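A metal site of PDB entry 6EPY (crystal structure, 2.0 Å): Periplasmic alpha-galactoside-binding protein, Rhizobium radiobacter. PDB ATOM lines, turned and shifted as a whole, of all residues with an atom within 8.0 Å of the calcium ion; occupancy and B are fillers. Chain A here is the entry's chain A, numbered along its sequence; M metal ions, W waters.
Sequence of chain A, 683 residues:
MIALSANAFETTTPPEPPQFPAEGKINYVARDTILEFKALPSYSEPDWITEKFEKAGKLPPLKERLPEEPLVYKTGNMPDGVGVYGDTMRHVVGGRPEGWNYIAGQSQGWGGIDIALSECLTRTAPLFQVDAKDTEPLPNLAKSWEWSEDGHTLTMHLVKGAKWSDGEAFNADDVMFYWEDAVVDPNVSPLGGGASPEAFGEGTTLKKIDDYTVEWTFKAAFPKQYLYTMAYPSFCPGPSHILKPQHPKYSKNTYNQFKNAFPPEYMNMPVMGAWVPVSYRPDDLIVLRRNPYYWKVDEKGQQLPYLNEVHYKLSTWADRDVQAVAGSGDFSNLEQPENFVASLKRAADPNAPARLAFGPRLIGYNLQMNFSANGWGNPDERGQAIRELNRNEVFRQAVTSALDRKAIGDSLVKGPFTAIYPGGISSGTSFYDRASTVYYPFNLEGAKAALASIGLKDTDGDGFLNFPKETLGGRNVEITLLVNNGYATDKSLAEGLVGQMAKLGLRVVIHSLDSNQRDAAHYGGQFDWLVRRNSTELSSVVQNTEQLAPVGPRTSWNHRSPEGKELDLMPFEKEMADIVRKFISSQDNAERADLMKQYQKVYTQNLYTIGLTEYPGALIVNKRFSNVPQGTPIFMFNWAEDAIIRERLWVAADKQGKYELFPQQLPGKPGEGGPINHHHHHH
The nearest printed residue that does not touch the calcium ion is Pro 186 (4.2 Å).
The calcium ion is bound by the backbone carbonyl oxygen (O) of Asp 185, the backbone carbonyl oxygen (O) of Val 188, the backbone carbonyl oxygen (O) of Val 183, water W1, the backbone carbonyl oxygen (O) of Ala 182, water W2 and water W3. The calcium ion has seven donor atoms within binding distance.
The side-chain carboxylate of Asp 185 is in hydrogen-bond range of the backbone NH of Asn 187 (3.0 Å). The backbone carbonyl oxygen (O) of Glu 180 sits at hydrogen-bond distance from the backbone NH (N) of Asp 185. The backbone NH (N) of Val 183 sits at hydrogen-bond distance from the backbone carbonyl oxygen (O) of Tyr 178 (2.9 Å).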
ATOM      1  N   ILE A 103     -15.614 -16.269 -10.978  1.00  0.00           N
ATOM      2  CA  ILE A 103     -15.609 -15.567 -12.270  1.00  0.00           C
ATOM      3  C   ILE A 103     -14.196 -15.042 -12.645  1.00  0.00           C
ATOM      4  O   ILE A 103     -13.949 -14.750 -13.815  1.00  0.00           O
ATOM      5  CB  ILE A 103     -16.720 -14.486 -12.371  1.00  0.00           C
ATOM      6  CG1 ILE A 103     -16.496 -13.346 -11.351  1.00  0.00           C
ATOM      7  CG2 ILE A 103     -18.117 -15.114 -12.241  1.00  0.00           C
ATOM      8  CD1 ILE A 103     -16.251 -12.019 -11.961  1.00  0.00           C
ATOM      9  N   TYR A 178     -20.649  -9.686 -15.430  1.00  0.00           N
ATOM     10  CA  TYR A 178     -19.972 -10.920 -15.825  1.00  0.00           C
ATOM     11  C   TYR A 178     -19.530 -10.830 -17.298  1.00  0.00           C
ATOM     12  O   TYR A 178     -18.376 -11.115 -17.608  1.00  0.00           O
ATOM     13  CB  TYR A 178     -20.858 -12.171 -15.589  1.00  0.00           C
ATOM     14  CG  TYR A 178     -20.202 -13.452 -16.087  1.00  0.00           C
ATOM     15  CD1 TYR A 178     -19.116 -13.999 -15.424  1.00  0.00           C
ATOM     16  CD2 TYR A 178     -20.615 -14.059 -17.281  1.00  0.00           C
ATOM     17  CE1 TYR A 178     -18.480 -15.155 -15.892  1.00  0.00           C
ATOM     18  CE2 TYR A 178     -19.993 -15.215 -17.763  1.00  0.00           C
ATOM     19  CZ  TYR A 178     -18.906 -15.740 -17.073  1.00  0.00           C
ATOM     20  OH  TYR A 178     -18.256 -16.874 -17.514  1.00  0.00           O
ATOM     21  N   TRP A 179     -20.463 -10.446 -18.197  1.00  0.00           N
ATOM     22  CA  TRP A 179     -20.171 -10.342 -19.626  1.00  0.00           C
ATOM     23  C   TRP A 179     -19.019  -9.380 -19.956  1.00  0.00           C
ATOM     24  O   TRP A 179     -18.053  -9.781 -20.595  1.00  0.00           O
ATOM     25  CB  TRP A 179     -21.443  -9.985 -20.441  1.00  0.00           C
ATOM     26  CG  TRP A 179     -21.168  -9.852 -21.908  1.00  0.00           C
ATOM     27  CD1 TRP A 179     -21.059  -8.696 -22.633  1.00  0.00           C
ATOM     28  CD2 TRP A 179     -20.802 -10.925 -22.809  1.00  0.00           C
ATOM     29  NE1 TRP A 179     -20.700  -8.977 -23.926  1.00  0.00           N
ATOM     30  CE2 TRP A 179     -20.552 -10.340 -24.069  1.00  0.00           C
ATOM     31  CE3 TRP A 179     -20.716 -12.319 -22.674  1.00  0.00           C
ATOM     32  CZ2 TRP A 179     -20.205 -11.098 -25.191  1.00  0.00           C
ATOM     33  CZ3 TRP A 179     -20.363 -13.078 -23.789  1.00  0.00           C
ATOM     34  CH2 TRP A 179     -20.098 -12.471 -25.022  1.00  0.00           C
ATOM     35  N   GLU A 180     -19.141  -8.105 -19.520  1.00  0.00           N
ATOM     36  CA  GLU A 180     -18.155  -7.066 -19.805  1.00  0.00           C
ATOM     37  C   GLU A 180     -16.851  -7.187 -19.024  1.00  0.00           C
ATOM     38  O   GLU A 180     -15.781  -7.097 -19.605  1.00  0.00           O
ATOM     39  CB  GLU A 180     -18.773  -5.667 -19.536  1.00  0.00           C
ATOM     40  CG  GLU A 180     -19.842  -5.241 -20.529  1.00  0.00           C
ATOM     41  CD  GLU A 180     -20.591  -3.947 -20.191  1.00  0.00           C
ATOM     42  OE1 GLU A 180     -20.167  -3.223 -19.256  1.00  0.00           O
ATOM     43  OE2 GLU A 180     -21.588  -3.660 -20.878  1.00  0.00           O
ATOM     44  N   ASP A 181     -16.938  -7.345 -17.692  1.00  0.00           N
ATOM     45  CA  ASP A 181     -15.792  -7.265 -16.820  1.00  0.00           C
ATOM     46  C   ASP A 181     -15.136  -8.623 -16.481  1.00  0.00           C
ATOM     47  O   ASP A 181     -14.074  -8.627 -15.846  1.00  0.00           O
ATOM     48  CB  ASP A 181     -16.162  -6.463 -15.568  1.00  0.00           C
ATOM     49  CG  ASP A 181     -16.499  -5.009 -15.921  1.00  0.00           C
ATOM     50  OD1 ASP A 181     -15.780  -4.400 -16.744  1.00  0.00           O
ATOM     51  OD2 ASP A 181     -17.558  -4.516 -15.457  1.00  0.00           O
ATOM     52  N   ALA A 182     -15.696  -9.742 -16.979  1.00  0.00           N
ATOM     53  CA  ALA A 182     -15.073 -11.063 -16.814  1.00  0.00           C
ATOM     54  C   ALA A 182     -14.861 -11.731 -18.168  1.00  0.00           C
ATOM     55  O   ALA A 182     -13.707 -12.029 -18.506  1.00  0.00           O
ATOM     56  CB  ALA A 182     -15.902 -11.967 -15.897  1.00  0.00           C
ATOM     57  N   VAL A 183     -15.930 -11.902 -18.972  1.00  0.00           N
ATOM     58  CA  VAL A 183     -15.828 -12.520 -20.306  1.00  0.00           C
ATOM     59  C   VAL A 183     -14.986 -11.650 -21.261  1.00  0.00           C
ATOM     60  O   VAL A 183     -13.867 -12.035 -21.592  1.00  0.00           O
ATOM     61  CB  VAL A 183     -17.198 -12.935 -20.933  1.00  0.00           C
ATOM     62  CG1 VAL A 183     -17.019 -13.514 -22.339  1.00  0.00           C
ATOM     63  CG2 VAL A 183     -17.899 -13.951 -20.038  1.00  0.00           C
ATOM     64  N   VAL A 184     -15.532 -10.466 -21.661  1.00  0.00           N
ATOM     65  CA  VAL A 184     -14.928  -9.538 -22.614  1.00  0.00           C
ATOM     66  C   VAL A 184     -13.542  -9.065 -22.112  1.00  0.00           C
ATOM     67  O   VAL A 184     -12.588  -9.104 -22.884  1.00  0.00           O
ATOM     68  CB  VAL A 184     -15.886  -8.365 -23.024  1.00  0.00           C
ATOM     69  CG1 VAL A 184     -15.184  -7.350 -23.933  1.00  0.00           C
ATOM     70  CG2 VAL A 184     -17.127  -8.906 -23.715  1.00  0.00           C
ATOM     71  N   ASP A 185     -13.435  -8.708 -20.820  1.00  0.00           N
ATOM     72  CA  ASP A 185     -12.182  -8.257 -20.220  1.00  0.00           C
ATOM     73  C   ASP A 185     -11.072  -9.318 -20.462  1.00  0.00           C
ATOM     74  O   ASP A 185     -11.240 -10.446 -20.039  1.00  0.00           O
ATOM     75  CB  ASP A 185     -12.372  -7.990 -18.716  1.00  0.00           C
ATOM     76  CG  ASP A 185     -11.245  -7.193 -18.073  1.00  0.00           C
ATOM     77  OD1 ASP A 185     -10.057  -7.553 -18.290  1.00  0.00           O
ATOM     78  OD2 ASP A 185     -11.554  -6.266 -17.291  1.00  0.00           O
ATOM     79  N   PRO A 186      -9.966  -8.992 -21.191  1.00  0.00           N
ATOM     80  CA  PRO A 186      -8.945 -10.020 -21.474  1.00  0.00           C
ATOM     81  C   PRO A 186      -8.026 -10.369 -20.301  1.00  0.00           C
ATOM     82  O   PRO A 186      -7.185 -11.269 -20.430  1.00  0.00           O
ATOM     83  CB  PRO A 186      -8.150  -9.417 -22.641  1.00  0.00           C
ATOM     84  CG  PRO A 186      -8.256  -7.931 -22.430  1.00  0.00           C
ATOM     85  CD  PRO A 186      -9.616  -7.681 -21.789  1.00  0.00           C
ATOM     86  N   ASN A 187      -8.180  -9.684 -19.166  1.00  0.00           N
ATOM     87  CA  ASN A 187      -7.373  -9.901 -17.959  1.00  0.00           C
ATOM     88  C   ASN A 187      -8.101 -10.707 -16.878  1.00  0.00           C
ATOM     89  O   ASN A 187      -7.546 -10.958 -15.816  1.00  0.00           O
ATOM     90  CB  ASN A 187      -6.868  -8.554 -17.440  1.00  0.00           C
ATOM     91  CG  ASN A 187      -5.908  -7.903 -18.380  1.00  0.00           C
ATOM     92  OD1 ASN A 187      -4.830  -8.430 -18.642  1.00  0.00           O
ATOM     93  ND2 ASN A 187      -6.312  -6.807 -18.966  1.00  0.00           N
ATOM     94  N   VAL A 188      -9.334 -11.134 -17.180  1.00  0.00           N
ATOM     95  CA  VAL A 188     -10.147 -11.942 -16.293  1.00  0.00           C
ATOM     96  C   VAL A 188     -10.546 -13.216 -17.050  1.00  0.00           C
ATOM     97  O   VAL A 188     -11.074 -13.123 -18.160  1.00  0.00           O
ATOM     98  CB  VAL A 188     -11.395 -11.175 -15.738  1.00  0.00           C
ATOM     99  CG1 VAL A 188     -12.131 -12.004 -14.691  1.00  0.00           C
ATOM    100  CG2 VAL A 188     -11.007  -9.824 -15.152  1.00  0.00           C
ATOM    101  N   SER A 189     -10.282 -14.382 -16.455  1.00  0.00           N
ATOM    102  CA  SER A 189     -10.630 -15.677 -17.066  1.00  0.00           C
ATOM    103  C   SER A 189     -11.408 -16.527 -16.060  1.00  0.00           C
ATOM    104  O   SER A 189     -10.831 -16.987 -15.072  1.00  0.00           O
ATOM    105  CB  SER A 189      -9.376 -16.418 -17.545  1.00  0.00           C
ATOM    106  OG  SER A 189      -8.791 -15.732 -18.641  1.00  0.00           O
ATOM    107  N   PRO A 190     -12.722 -16.749 -16.277  1.00  0.00           N
ATOM    108  CA  PRO A 190     -13.503 -17.574 -15.324  1.00  0.00           C
ATOM    109  C   PRO A 190     -12.988 -19.009 -15.180  1.00  0.00           C
ATOM    110  O   PRO A 190     -12.248 -19.492 -16.032  1.00  0.00           O
ATOM    111  CB  PRO A 190     -14.928 -17.559 -15.921  1.00  0.00           C
ATOM    112  CG  PRO A 190     -14.964 -16.290 -16.746  1.00  0.00           C
ATOM    113  CD  PRO A 190     -13.576 -16.237 -17.364  1.00  0.00           C
ATOM    114  N   GLY A 194     -12.591 -22.127 -20.095  1.00  0.00           N
ATOM    115  CA  GLY A 194     -13.455 -21.653 -21.171  1.00  0.00           C
ATOM    116  C   GLY A 194     -13.877 -20.201 -20.937  1.00  0.00           C
ATOM    117  O   GLY A 194     -13.124 -19.412 -20.354  1.00  0.00           O
ATOM    118  N   ALA A 195     -15.099 -19.857 -21.387  1.00  0.00           N
ATOM    119  CA  ALA A 195     -15.710 -18.530 -21.247  1.00  0.00           C
ATOM    120  C   ALA A 195     -14.901 -17.369 -21.889  1.00  0.00           C
ATOM    121  O   ALA A 195     -14.949 -16.226 -21.411  1.00  0.00           O
ATOM    122  CB  ALA A 195     -16.046 -18.225 -19.771  1.00  0.00           C
ATOM    123  N   SER A 196     -14.221 -17.641 -23.031  1.00  0.00           N
ATOM    124  CA  SER A 196     -13.577 -16.568 -23.790  1.00  0.00           C
ATOM    125  C   SER A 196     -14.734 -15.876 -24.582  1.00  0.00           C
ATOM    126  O   SER A 196     -15.795 -16.503 -24.727  1.00  0.00           O
ATOM    127  CB  SER A 196     -12.512 -17.114 -24.740  1.00  0.00           C
ATOM    128  OG  SER A 196     -13.061 -17.871 -25.803  1.00  0.00           O
ATOM    129  N   PRO A 197     -14.597 -14.621 -25.074  1.00  0.00           N
ATOM    130  CA  PRO A 197     -15.718 -14.009 -25.829  1.00  0.00           C
ATOM    131  C   PRO A 197     -16.196 -14.834 -27.041  1.00  0.00           C
ATOM    132  O   PRO A 197     -17.399 -14.927 -27.295  1.00  0.00           O
ATOM    133  CB  PRO A 197     -15.157 -12.639 -26.256  1.00  0.00           C
ATOM    134  CG  PRO A 197     -14.042 -12.360 -25.332  1.00  0.00           C
ATOM    135  CD  PRO A 197     -13.441 -13.693 -24.982  1.00  0.00           C
ATOM    136  N   ARG A 554      -8.975 -19.022 -28.316  1.00  0.00           N
ATOM    137  CA  ARG A 554      -8.757 -19.691 -27.028  1.00  0.00           C
ATOM    138  C   ARG A 554      -9.778 -20.804 -26.709  1.00  0.00           C
ATOM    139  O   ARG A 554      -9.825 -21.285 -25.573  1.00  0.00           O
ATOM    140  CB  ARG A 554      -8.680 -18.650 -25.883  1.00  0.00           C
ATOM    141  CG  ARG A 554      -7.461 -17.737 -26.015  1.00  0.00           C
ATOM    142  CD  ARG A 554      -7.403 -16.635 -24.990  1.00  0.00           C
ATOM    143  NE  ARG A 554      -6.165 -15.864 -25.123  1.00  0.00           N
ATOM    144  CZ  ARG A 554      -5.957 -14.890 -26.007  1.00  0.00           C
ATOM    145  NH1 ARG A 554      -6.909 -14.552 -26.875  1.00  0.00           N
ATOM    146  NH2 ARG A 554      -4.803 -14.244 -26.031  1.00  0.00           N
ATOM    147  N   GLU A 563      -1.004 -14.008 -26.049  1.00  0.00           N
ATOM    148  CA  GLU A 563      -1.486 -12.624 -26.059  1.00  0.00           C
ATOM    149  C   GLU A 563      -0.309 -11.654 -26.276  1.00  0.00           C
ATOM    150  O   GLU A 563       0.654 -11.701 -25.519  1.00  0.00           O
ATOM    151  CB  GLU A 563      -2.334 -12.260 -24.817  1.00  0.00           C
ATOM    152  CG  GLU A 563      -3.359 -11.181 -25.107  1.00  0.00           C
ATOM    153  CD  GLU A 563      -4.159 -10.665 -23.926  1.00  0.00           C
ATOM    154  OE1 GLU A 563      -4.014  -9.468 -23.575  1.00  0.00           O
ATOM    155  OE2 GLU A 563      -4.959 -11.451 -23.353  1.00  0.00           O
HETATM  156 CA    CA M   1     -12.040 -12.575 -20.212  1.00  0.00          CA
HETATM  157  O   HOH W   1     -12.788 -14.777 -20.597  1.00  0.00           O
HETATM  158  O   HOH W   2     -11.282 -12.362 -22.532  1.00  0.00           O
HETATM  159  O   HOH W   3      -9.660 -13.782 -20.560  1.00  0.00           O
